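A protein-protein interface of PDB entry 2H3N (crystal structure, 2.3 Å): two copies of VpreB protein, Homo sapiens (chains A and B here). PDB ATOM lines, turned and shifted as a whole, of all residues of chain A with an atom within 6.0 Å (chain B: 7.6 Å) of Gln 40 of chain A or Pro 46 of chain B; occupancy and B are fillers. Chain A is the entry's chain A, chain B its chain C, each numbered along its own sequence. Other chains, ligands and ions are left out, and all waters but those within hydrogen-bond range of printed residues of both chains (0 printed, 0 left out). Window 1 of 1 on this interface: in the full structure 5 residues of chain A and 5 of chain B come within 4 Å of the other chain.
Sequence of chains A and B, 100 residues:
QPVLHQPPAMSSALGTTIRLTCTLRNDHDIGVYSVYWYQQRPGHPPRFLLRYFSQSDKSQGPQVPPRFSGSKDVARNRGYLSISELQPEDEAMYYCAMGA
Among the printed residues, pairs that only touch across the chains: Gln 40 of chain A with Pro 46 of chain B, Gln 40 of chain A with Tyr 95 of chain B, His 44 of chain A with Tyr 95 of chain B, Pro 45 of chain A with Tyr 95 of chain B, Pro 46 of chain A with Pro 46 of chain B, Pro 46 of chain A with Tyr 95 of chain B, Tyr 95 of chain A with His 44 of chain B, Tyr 95 of chain A with Pro 45 of chain B and Tyr 95 of chain A with Pro 46 of chain B.
Gln 40 of chain A touches three residues of chain B. Of the printed residues of chain A, Pro 46 of chain B touches Gln 40 (3.9 Å), Pro 46 (3.995 Å) and Tyr 95 (3.4 Å). Printed residues of chain A within 4 Å of Pro 45 of chain B: Tyr 95. Of the printed residues of chain B, His 44 of chain A touches Tyr 95 (3.6 Å). Of the printed residues of chain A, Tyr 95 of chain B touches Gln 40 (3.8 Å), His 44 (3.6 Å), Pro 45 (3.4 Å) and Pro 46 (3.8 Å). Of the printed residues of chain B, Tyr 95 of chain A touches His 44, Pro 45 and Pro 46. The nearest residue of chain B that does not touch Gln 40 of chain A is His 44 of chain B (5.1 Å). The nearest printed residue of chain A that does not touch Pro 46 of chain B is Met 93 of chain A (7.0 Å). The nearest printed residue of chain B that does not touch Pro 45 of chain A is Met 93 of chain B (5.9 Å).
The side-chain amide nitrogen (NE2) of Gln 40 of chain B sits at hydrogen-bond distance from the side-chain amide oxygen (OE1) of Gln 40 of chain A (2.8 Å).
Of the 13 printed residues of chain B, 5 touch a printed residue of chain A. Printed residues of chain A that touch a printed residue of chain B: Gln 40, His 44, Pro 45, Pro 46 and Tyr 95. Among the printed residues, 10 pairs touch across the chains. Among the printed residues, no Asp or Glu carboxylate lies within 4 Å of a Lys or Arg side-chain nitrogen of the other chain.
The side-chain amide nitrogen of Gln 40 of chain A sits at hydrogen-bond distance from the backbone carbonyl oxygen of His 44 of chain A (2.8 Å). The backbone NH (N) of Tyr 38 of chain A lies within hydrogen-bond range of the backbone carbonyl oxygen (O) of Tyr 95 of chain A, at 2.8 Å. O of Met 93 of chain A lies within hydrogen-bond range of N of Gln 40 of chain A (2.9 Å). O of Tyr 95 of chain B sits at hydrogen-bond distance from N of Tyr 38 of chain B (2.8 Å). The side-chain amide nitrogen (NE2) of Gln 40 of chain B sits at hydrogen-bond distance from the backbone carbonyl oxygen (O) of His 44 of chain B (3.0 Å). The backbone carbonyl oxygen of Met 93 of chain B sits at hydrogen-bond distance from the backbone NH of Gln 40 of chain B, 3.0 Å away.
Gln 40 of chain B touches its own counterpart, Gln 40 of chain A. Gln 40 of chain A touches Tyr 95 of chain B, but with the chains exchanged Tyr 95 of chain A does not touch Gln 40 of chain B (4.01 Å). His 44 of chain A touches Tyr 95 of chain B, and with the chains exchanged Tyr 95 of chain A touches His 44 of chain B. Pro 46 of chain A touches its own counterpart, Pro 46 of chain B. Positions printed for both chains: 38, 39, 40, 41, 44, 45, 46, 47, 93 and 95.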
ATOM      1  N   TYR A  38     -18.028 -16.953  16.725  1.00  0.00           N
ATOM      2  CA  TYR A  38     -17.790 -15.679  16.057  1.00  0.00           C
ATOM      3  C   TYR A  38     -18.376 -15.706  14.658  1.00  0.00           C
ATOM      4  O   TYR A  38     -18.362 -16.745  13.990  1.00  0.00           O
ATOM      5  CB  TYR A  38     -16.288 -15.383  15.946  1.00  0.00           C
ATOM      6  CG  TYR A  38     -15.543 -15.300  17.261  1.00  0.00           C
ATOM      7  CD1 TYR A  38     -15.129 -16.449  17.927  1.00  0.00           C
ATOM      8  CD2 TYR A  38     -15.249 -14.065  17.837  1.00  0.00           C
ATOM      9  CE1 TYR A  38     -14.435 -16.370  19.135  1.00  0.00           C
ATOM     10  CE2 TYR A  38     -14.566 -13.975  19.036  1.00  0.00           C
ATOM     11  CZ  TYR A  38     -14.159 -15.129  19.679  1.00  0.00           C
ATOM     12  OH  TYR A  38     -13.465 -15.027  20.861  1.00  0.00           O
ATOM     13  N   GLN A  39     -18.882 -14.558  14.217  1.00  0.00           N
ATOM     14  CA  GLN A  39     -19.464 -14.422  12.886  1.00  0.00           C
ATOM     15  C   GLN A  39     -18.604 -13.466  12.069  1.00  0.00           C
ATOM     16  O   GLN A  39     -18.132 -12.455  12.581  1.00  0.00           O
ATOM     17  CB  GLN A  39     -20.894 -13.876  12.978  1.00  0.00           C
ATOM     18  CG  GLN A  39     -21.395 -13.205  11.710  1.00  0.00           C
ATOM     19  CD  GLN A  39     -22.780 -12.588  11.875  1.00  0.00           C
ATOM     20  OE1 GLN A  39     -23.805 -13.268  11.735  1.00  0.00           O
ATOM     21  NE2 GLN A  39     -22.816 -11.297  12.194  1.00  0.00           N
ATOM     22  N   GLN A  40     -18.406 -13.798  10.798  1.00  0.00           N
ATOM     23  CA  GLN A  40     -17.612 -12.966   9.915  1.00  0.00           C
ATOM     24  C   GLN A  40     -18.187 -12.957   8.500  1.00  0.00           C
ATOM     25  O   GLN A  40     -18.189 -13.971   7.809  1.00  0.00           O
ATOM     26  CB  GLN A  40     -16.148 -13.444   9.880  1.00  0.00           C
ATOM     27  CG  GLN A  40     -15.314 -12.704   8.847  1.00  0.00           C
ATOM     28  CD  GLN A  40     -13.827 -13.016   8.892  1.00  0.00           C
ATOM     29  OE1 GLN A  40     -13.409 -14.177   8.917  1.00  0.00           O
ATOM     30  NE2 GLN A  40     -13.017 -11.969   8.878  1.00  0.00           N
ATOM     31  N   ARG A  41     -18.689 -11.793   8.102  1.00  0.00           N
ATOM     32  CA  ARG A  41     -19.238 -11.576   6.776  1.00  0.00           C
ATOM     33  C   ARG A  41     -18.125 -11.126   5.842  1.00  0.00           C
ATOM     34  O   ARG A  41     -17.168 -10.467   6.266  1.00  0.00           O
ATOM     35  CB  ARG A  41     -20.304 -10.491   6.832  1.00  0.00           C
ATOM     36  CG  ARG A  41     -21.469 -10.847   7.705  1.00  0.00           C
ATOM     37  CD  ARG A  41     -22.201  -9.611   8.129  1.00  0.00           C
ATOM     38  NE  ARG A  41     -23.382  -9.937   8.912  1.00  0.00           N
ATOM     39  CZ  ARG A  41     -24.162  -9.032   9.489  1.00  0.00           C
ATOM     40  NH1 ARG A  41     -23.876  -7.742   9.372  1.00  0.00           N
ATOM     41  NH2 ARG A  41     -25.230  -9.417  10.176  1.00  0.00           N
ATOM     42  N   PRO A  42     -18.235 -11.478   4.551  1.00  0.00           N
ATOM     43  CA  PRO A  42     -17.238 -11.105   3.548  1.00  0.00           C
ATOM     44  C   PRO A  42     -16.898  -9.616   3.631  1.00  0.00           C
ATOM     45  O   PRO A  42     -17.782  -8.767   3.541  1.00  0.00           O
ATOM     46  CB  PRO A  42     -17.935 -11.465   2.235  1.00  0.00           C
ATOM     47  CG  PRO A  42     -18.703 -12.700   2.617  1.00  0.00           C
ATOM     48  CD  PRO A  42     -19.320 -12.270   3.940  1.00  0.00           C
ATOM     49  N   HIS A  44     -15.475  -8.144   6.291  1.00  0.00           N
ATOM     50  CA  HIS A  44     -15.519  -7.633   7.658  1.00  0.00           C
ATOM     51  C   HIS A  44     -14.705  -8.422   8.660  1.00  0.00           C
ATOM     52  O   HIS A  44     -14.363  -9.583   8.447  1.00  0.00           O
ATOM     53  CB  HIS A  44     -16.967  -7.648   8.172  1.00  0.00           C
ATOM     54  CG  HIS A  44     -17.882  -6.715   7.449  1.00  0.00           C
ATOM     55  ND1 HIS A  44     -18.157  -5.442   7.899  1.00  0.00           N
ATOM     56  CD2 HIS A  44     -18.571  -6.864   6.291  1.00  0.00           C
ATOM     57  CE1 HIS A  44     -18.972  -4.844   7.050  1.00  0.00           C
ATOM     58  NE2 HIS A  44     -19.240  -5.684   6.066  1.00  0.00           N
ATOM     59  N   PRO A  45     -14.389  -7.791   9.794  1.00  0.00           N
ATOM     60  CA  PRO A  45     -13.622  -8.452  10.844  1.00  0.00           C
ATOM     61  C   PRO A  45     -14.522  -9.469  11.556  1.00  0.00           C
ATOM     62  O   PRO A  45     -15.746  -9.430  11.446  1.00  0.00           O
ATOM     63  CB  PRO A  45     -13.291  -7.310  11.803  1.00  0.00           C
ATOM     64  CG  PRO A  45     -13.170  -6.134  10.872  1.00  0.00           C
ATOM     65  CD  PRO A  45     -14.434  -6.340  10.049  1.00  0.00           C
ATOM     66  N   PRO A  46     -13.919 -10.401  12.290  1.00  0.00           N
ATOM     67  CA  PRO A  46     -14.747 -11.377  13.000  1.00  0.00           C
ATOM     68  C   PRO A  46     -15.557 -10.633  14.076  1.00  0.00           C
ATOM     69  O   PRO A  46     -15.109  -9.626  14.607  1.00  0.00           O
ATOM     70  CB  PRO A  46     -13.714 -12.318  13.608  1.00  0.00           C
ATOM     71  CG  PRO A  46     -12.622 -12.313  12.572  1.00  0.00           C
ATOM     72  CD  PRO A  46     -12.501 -10.825  12.300  1.00  0.00           C
ATOM     73  N   ARG A  47     -16.758 -11.107  14.379  1.00  0.00           N
ATOM     74  CA  ARG A  47     -17.560 -10.457  15.411  1.00  0.00           C
ATOM     75  C   ARG A  47     -17.923 -11.462  16.497  1.00  0.00           C
ATOM     76  O   ARG A  47     -18.471 -12.522  16.207  1.00  0.00           O
ATOM     77  CB  ARG A  47     -18.832  -9.856  14.810  1.00  0.00           C
ATOM     78  CG  ARG A  47     -19.768  -9.238  15.849  1.00  0.00           C
ATOM     79  CD  ARG A  47     -21.150  -8.927  15.269  1.00  0.00           C
ATOM     80  NE  ARG A  47     -22.026  -8.266  16.239  1.00  0.00           N
ATOM     81  CZ  ARG A  47     -22.011  -6.961  16.506  1.00  0.00           C
ATOM     82  NH1 ARG A  47     -21.167  -6.155  15.873  1.00  0.00           N
ATOM     83  NH2 ARG A  47     -22.842  -6.460  17.412  1.00  0.00           N
ATOM     84  N   GLU A  91     -26.011 -14.473   6.565  1.00  0.00           N
ATOM     85  CA  GLU A  91     -25.130 -15.232   5.678  1.00  0.00           C
ATOM     86  C   GLU A  91     -23.681 -14.843   5.977  1.00  0.00           C
ATOM     87  O   GLU A  91     -23.268 -13.714   5.745  1.00  0.00           O
ATOM     88  CB  GLU A  91     -25.461 -14.942   4.214  1.00  0.00           C
ATOM     89  CG  GLU A  91     -26.216 -16.063   3.504  1.00  0.00           C
ATOM     90  CD  GLU A  91     -26.345 -15.824   2.004  1.00  0.00           C
ATOM     91  OE1 GLU A  91     -25.462 -15.150   1.427  1.00  0.00           O
ATOM     92  OE2 GLU A  91     -27.318 -16.324   1.399  1.00  0.00           O
ATOM     93  N   ALA A  92     -22.905 -15.788   6.482  1.00  0.00           N
ATOM     94  CA  ALA A  92     -21.534 -15.486   6.839  1.00  0.00           C
ATOM     95  C   ALA A  92     -20.821 -16.731   7.305  1.00  0.00           C
ATOM     96  O   ALA A  92     -21.425 -17.796   7.423  1.00  0.00           O
ATOM     97  CB  ALA A  92     -21.516 -14.440   7.968  1.00  0.00           C
ATOM     98  N   MET A  93     -19.529 -16.584   7.565  1.00  0.00           N
ATOM     99  CA  MET A  93     -18.728 -17.679   8.090  1.00  0.00           C
ATOM    100  C   MET A  93     -18.904 -17.664   9.605  1.00  0.00           C
ATOM    101  O   MET A  93     -18.951 -16.593  10.208  1.00  0.00           O
ATOM    102  CB  MET A  93     -17.248 -17.469   7.769  1.00  0.00           C
ATOM    103  CG  MET A  93     -16.839 -17.857   6.367  1.00  0.00           C
ATOM    104  SD  MET A  93     -17.069 -19.633   6.126  1.00  0.00           S
ATOM    105  CE  MET A  93     -15.816 -20.278   7.148  1.00  0.00           C
ATOM    106  N   TYR A  94     -19.004 -18.845  10.213  1.00  0.00           N
ATOM    107  CA  TYR A  94     -19.147 -18.957  11.661  1.00  0.00           C
ATOM    108  C   TYR A  94     -18.052 -19.829  12.225  1.00  0.00           C
ATOM    109  O   TYR A  94     -17.959 -21.000  11.882  1.00  0.00           O
ATOM    110  CB  TYR A  94     -20.500 -19.569  12.039  1.00  0.00           C
ATOM    111  CG  TYR A  94     -21.649 -18.644  11.767  1.00  0.00           C
ATOM    112  CD1 TYR A  94     -22.256 -18.604  10.515  1.00  0.00           C
ATOM    113  CD2 TYR A  94     -22.067 -17.731  12.732  1.00  0.00           C
ATOM    114  CE1 TYR A  94     -23.236 -17.678  10.229  1.00  0.00           C
ATOM    115  CE2 TYR A  94     -23.046 -16.796  12.455  1.00  0.00           C
ATOM    116  CZ  TYR A  94     -23.622 -16.770  11.199  1.00  0.00           C
ATOM    117  OH  TYR A  94     -24.532 -15.793  10.879  1.00  0.00           O
ATOM    118  N   TYR A  95     -17.219 -19.266  13.091  1.00  0.00           N
ATOM    119  CA  TYR A  95     -16.151 -20.048  13.693  1.00  0.00           C
ATOM    120  C   TYR A  95     -16.411 -20.233  15.182  1.00  0.00           C
ATOM    121  O   TYR A  95     -17.018 -19.387  15.824  1.00  0.00           O
ATOM    122  CB  TYR A  95     -14.795 -19.351  13.537  1.00  0.00           C
ATOM    123  CG  TYR A  95     -14.416 -18.963  12.128  1.00  0.00           C
ATOM    124  CD1 TYR A  95     -14.620 -17.666  11.658  1.00  0.00           C
ATOM    125  CD2 TYR A  95     -13.856 -19.895  11.262  1.00  0.00           C
ATOM    126  CE1 TYR A  95     -14.271 -17.305  10.349  1.00  0.00           C
ATOM    127  CE2 TYR A  95     -13.503 -19.549   9.952  1.00  0.00           C
ATOM    128  CZ  TYR A  95     -13.714 -18.252   9.502  1.00  0.00           C
ATOM    129  OH  TYR A  95     -13.364 -17.905   8.209  1.00  0.00           O
ATOM    130  N   TRP B  37      -3.685 -11.356  18.850  1.00  0.00           N
ATOM    131  CA  TRP B  37      -3.442 -11.055  17.452  1.00  0.00           C
ATOM    132  C   TRP B  37      -3.765 -12.251  16.581  1.00  0.00           C
ATOM    133  O   TRP B  37      -3.402 -13.379  16.898  1.00  0.00           O
ATOM    134  CB  TRP B  37      -1.989 -10.627  17.232  1.00  0.00           C
ATOM    135  CG  TRP B  37      -1.696  -9.247  17.718  1.00  0.00           C
ATOM    136  CD1 TRP B  37      -1.164  -8.897  18.924  1.00  0.00           C
ATOM    137  CD2 TRP B  37      -1.899  -8.021  16.999  1.00  0.00           C
ATOM    138  NE1 TRP B  37      -1.013  -7.533  18.999  1.00  0.00           N
ATOM    139  CE2 TRP B  37      -1.456  -6.972  17.831  1.00  0.00           C
ATOM    140  CE3 TRP B  37      -2.408  -7.714  15.731  1.00  0.00           C
ATOM    141  CZ2 TRP B  37      -1.505  -5.628  17.439  1.00  0.00           C
ATOM    142  CZ3 TRP B  37      -2.458  -6.377  15.336  1.00  0.00           C
ATOM    143  CH2 TRP B  37      -2.007  -5.353  16.188  1.00  0.00           C
ATOM    144  N   TYR B  38      -4.447 -11.992  15.476  1.00  0.00           N
ATOM    145  CA  TYR B  38      -4.826 -13.035  14.541  1.00  0.00           C
ATOM    146  C   TYR B  38      -4.396 -12.639  13.136  1.00  0.00           C
ATOM    147  O   TYR B  38      -4.367 -11.457  12.810  1.00  0.00           O
ATOM    148  CB  TYR B  38      -6.341 -13.234  14.569  1.00  0.00           C
ATOM    149  CG  TYR B  38      -6.878 -13.609  15.933  1.00  0.00           C
ATOM    150  CD1 TYR B  38      -7.072 -12.645  16.923  1.00  0.00           C
ATOM    151  CD2 TYR B  38      -7.157 -14.937  16.247  1.00  0.00           C
ATOM    152  CE1 TYR B  38      -7.528 -12.999  18.195  1.00  0.00           C
ATOM    153  CE2 TYR B  38      -7.615 -15.300  17.515  1.00  0.00           C
ATOM    154  CZ  TYR B  38      -7.800 -14.326  18.480  1.00  0.00           C
ATOM    155  OH  TYR B  38      -8.266 -14.675  19.724  1.00  0.00           O
ATOM    156  N   GLN B  39      -4.057 -13.638  12.322  1.00  0.00           N
ATOM    157  CA  GLN B  39      -3.649 -13.452  10.928  1.00  0.00           C
ATOM    158  C   GLN B  39      -4.713 -14.145  10.077  1.00  0.00           C
ATOM    159  O   GLN B  39      -5.270 -15.167  10.486  1.00  0.00           O
ATOM    160  CB  GLN B  39      -2.285 -14.109  10.675  1.00  0.00           C
ATOM    161  CG  GLN B  39      -1.857 -14.198   9.209  1.00  0.00           C
ATOM    162  CD  GLN B  39      -0.591 -15.036   9.021  1.00  0.00           C
ATOM    163  OE1 GLN B  39       0.520 -14.515   9.034  1.00  0.00           O
ATOM    164  NE2 GLN B  39      -0.761 -16.343   8.862  1.00  0.00           N
ATOM    165  N   GLN B  40      -4.992 -13.596   8.898  1.00  0.00           N
ATOM    166  CA  GLN B  40      -5.989 -14.189   8.021  1.00  0.00           C
ATOM    167  C   GLN B  40      -5.712 -13.942   6.550  1.00  0.00           C
ATOM    168  O   GLN B  40      -5.553 -12.807   6.112  1.00  0.00           O
ATOM    169  CB  GLN B  40      -7.387 -13.670   8.373  1.00  0.00           C
ATOM    170  CG  GLN B  40      -8.493 -14.276   7.516  1.00  0.00           C
ATOM    171  CD  GLN B  40      -9.891 -13.868   7.960  1.00  0.00           C
ATOM    172  OE1 GLN B  40     -10.166 -12.693   8.171  1.00  0.00           O
ATOM    173  NE2 GLN B  40     -10.781 -14.841   8.088  1.00  0.00           N
ATOM    174  N   ARG B  41      -5.644 -15.023   5.784  1.00  0.00           N
ATOM    175  CA  ARG B  41      -5.405 -14.906   4.358  1.00  0.00           C
ATOM    176  C   ARG B  41      -6.733 -15.077   3.632  1.00  0.00           C
ATOM    177  O   ARG B  41      -7.686 -15.638   4.177  1.00  0.00           O
ATOM    178  CB  ARG B  41      -4.383 -15.952   3.894  1.00  0.00           C
ATOM    179  CG  ARG B  41      -3.015 -15.820   4.580  1.00  0.00           C
ATOM    180  CD  ARG B  41      -1.904 -16.518   3.802  1.00  0.00           C
ATOM    181  NE  ARG B  41      -0.597 -16.377   4.454  1.00  0.00           N
ATOM    182  CZ  ARG B  41      -0.242 -16.998   5.578  1.00  0.00           C
ATOM    183  NH1 ARG B  41      -1.092 -17.814   6.186  1.00  0.00           N
ATOM    184  NH2 ARG B  41       0.968 -16.814   6.089  1.00  0.00           N
ATOM    185  N   HIS B  44      -9.490 -17.997   4.074  1.00  0.00           N
ATOM    186  CA  HIS B  44      -8.988 -18.881   5.122  1.00  0.00           C
ATOM    187  C   HIS B  44      -9.566 -18.462   6.468  1.00  0.00           C
ATOM    188  O   HIS B  44     -10.128 -17.377   6.610  1.00  0.00           O
ATOM    189  CB  HIS B  44      -7.460 -18.798   5.192  1.00  0.00           C
ATOM    190  CG  HIS B  44      -6.750 -19.502   4.077  1.00  0.00           C
ATOM    191  ND1 HIS B  44      -6.566 -20.870   4.056  1.00  0.00           N
ATOM    192  CD2 HIS B  44      -6.138 -19.028   2.962  1.00  0.00           C
ATOM    193  CE1 HIS B  44      -5.870 -21.203   2.986  1.00  0.00           C
ATOM    194  NE2 HIS B  44      -5.598 -20.104   2.304  1.00  0.00           N
ATOM    195  N   PRO B  45      -9.452 -19.331   7.479  1.00  0.00           N
ATOM    196  CA  PRO B  45      -9.978 -18.974   8.793  1.00  0.00           C
ATOM    197  C   PRO B  45      -8.981 -18.075   9.514  1.00  0.00           C
ATOM    198  O   PRO B  45      -7.804 -18.015   9.156  1.00  0.00           O
ATOM    199  CB  PRO B  45     -10.098 -20.328   9.507  1.00  0.00           C
ATOM    200  CG  PRO B  45     -10.213 -21.317   8.379  1.00  0.00           C
ATOM    201  CD  PRO B  45      -9.201 -20.777   7.402  1.00  0.00           C
ATOM    202  N   PRO B  46      -9.446 -17.347  10.528  1.00  0.00           N
ATOM    203  CA  PRO B  46      -8.560 -16.466  11.292  1.00  0.00           C
ATOM    204  C   PRO B  46      -7.583 -17.377  12.029  1.00  0.00           C
ATOM    205  O   PRO B  46      -7.983 -18.424  12.530  1.00  0.00           O
ATOM    206  CB  PRO B  46      -9.515 -15.768  12.242  1.00  0.00           C
ATOM    207  CG  PRO B  46     -10.764 -15.650  11.400  1.00  0.00           C
ATOM    208  CD  PRO B  46     -10.859 -17.041  10.813  1.00  0.00           C
ATOM    209  N   ARG B  47      -6.311 -16.999  12.090  1.00  0.00           N
ATOM    210  CA  ARG B  47      -5.333 -17.842  12.758  1.00  0.00           C
ATOM    211  C   ARG B  47      -4.699 -17.134  13.943  1.00  0.00           C
ATOM    212  O   ARG B  47      -4.012 -16.123  13.777  1.00  0.00           O
ATOM    213  CB  ARG B  47      -4.255 -18.267  11.758  1.00  0.00           C
ATOM    214  CG  ARG B  47      -3.248 -19.259  12.295  1.00  0.00           C
ATOM    215  CD  ARG B  47      -2.531 -19.960  11.151  1.00  0.00           C
ATOM    216  NE  ARG B  47      -1.533 -20.896  11.643  1.00  0.00           N
ATOM    217  CZ  ARG B  47      -0.357 -20.528  12.135  1.00  0.00           C
ATOM    218  NH1 ARG B  47      -0.034 -19.239  12.189  1.00  0.00           N
ATOM    219  NH2 ARG B  47       0.486 -21.450  12.578  1.00  0.00           N
ATOM    220  N   PHE B  48      -4.940 -17.676  15.136  1.00  0.00           N
ATOM    221  CA  PHE B  48      -4.393 -17.131  16.376  1.00  0.00           C
ATOM    222  C   PHE B  48      -2.868 -17.104  16.321  1.00  0.00           C
ATOM    223  O   PHE B  48      -2.219 -18.147  16.271  1.00  0.00           O
ATOM    224  CB  PHE B  48      -4.858 -17.969  17.582  1.00  0.00           C
ATOM    225  CG  PHE B  48      -4.163 -17.622  18.877  1.00  0.00           C
ATOM    226  CD1 PHE B  48      -4.324 -16.373  19.462  1.00  0.00           C
ATOM    227  CD2 PHE B  48      -3.322 -18.542  19.493  1.00  0.00           C
ATOM    228  CE1 PHE B  48      -3.648 -16.042  20.650  1.00  0.00           C
ATOM    229  CE2 PHE B  48      -2.645 -18.221  20.674  1.00  0.00           C
ATOM    230  CZ  PHE B  48      -2.809 -16.970  21.252  1.00  0.00           C
ATOM    231  N   LEU B  49      -2.299 -15.903  16.319  1.00  0.00           N
ATOM    232  CA  LEU B  49      -0.847 -15.761  16.282  1.00  0.00           C
ATOM    233  C   LEU B  49      -0.228 -15.779  17.671  1.00  0.00           C
ATOM    234  O   LEU B  49       0.706 -16.530  17.922  1.00  0.00           O
ATOM    235  CB  LEU B  49      -0.447 -14.455  15.598  1.00  0.00           C
ATOM    236  CG  LEU B  49      -0.753 -14.281  14.113  1.00  0.00           C
ATOM    237  CD1 LEU B  49      -0.502 -12.836  13.724  1.00  0.00           C
ATOM    238  CD2 LEU B  49       0.109 -15.228  13.288  1.00  0.00           C
ATOM    239  N   MET B  93      -4.314 -10.018   6.368  1.00  0.00           N
ATOM    240  CA  MET B  93      -5.003  -9.095   7.274  1.00  0.00           C
ATOM    241  C   MET B  93      -4.599  -9.488   8.688  1.00  0.00           C
ATOM    242  O   MET B  93      -4.428 -10.672   8.963  1.00  0.00           O
ATOM    243  CB  MET B  93      -6.523  -9.250   7.164  1.00  0.00           C
ATOM    244  CG  MET B  93      -7.198  -8.442   6.068  1.00  0.00           C
ATOM    245  SD  MET B  93      -7.234  -6.664   6.371  1.00  0.00           S
ATOM    246  CE  MET B  93      -8.089  -6.581   7.966  1.00  0.00           C
ATOM    247  N   TYR B  95      -5.718  -8.871  12.816  1.00  0.00           N
ATOM    248  CA  TYR B  95      -6.724  -8.338  13.742  1.00  0.00           C
ATOM    249  C   TYR B  95      -6.259  -8.436  15.184  1.00  0.00           C
ATOM    250  O   TYR B  95      -5.663  -9.437  15.575  1.00  0.00           O
ATOM    251  CB  TYR B  95      -8.038  -9.130  13.645  1.00  0.00           C
ATOM    252  CG  TYR B  95      -8.748  -9.068  12.317  1.00  0.00           C
ATOM    253  CD1 TYR B  95      -8.737 -10.156  11.449  1.00  0.00           C
ATOM    254  CD2 TYR B  95      -9.449  -7.927  11.934  1.00  0.00           C
ATOM    255  CE1 TYR B  95      -9.416 -10.114  10.238  1.00  0.00           C
ATOM    256  CE2 TYR B  95     -10.129  -7.873  10.718  1.00  0.00           C
ATOM    257  CZ  TYR B  95     -10.106  -8.968   9.880  1.00  0.00           C
ATOM    258  OH  TYR B  95     -10.792  -8.941   8.696  1.00  0.00           O
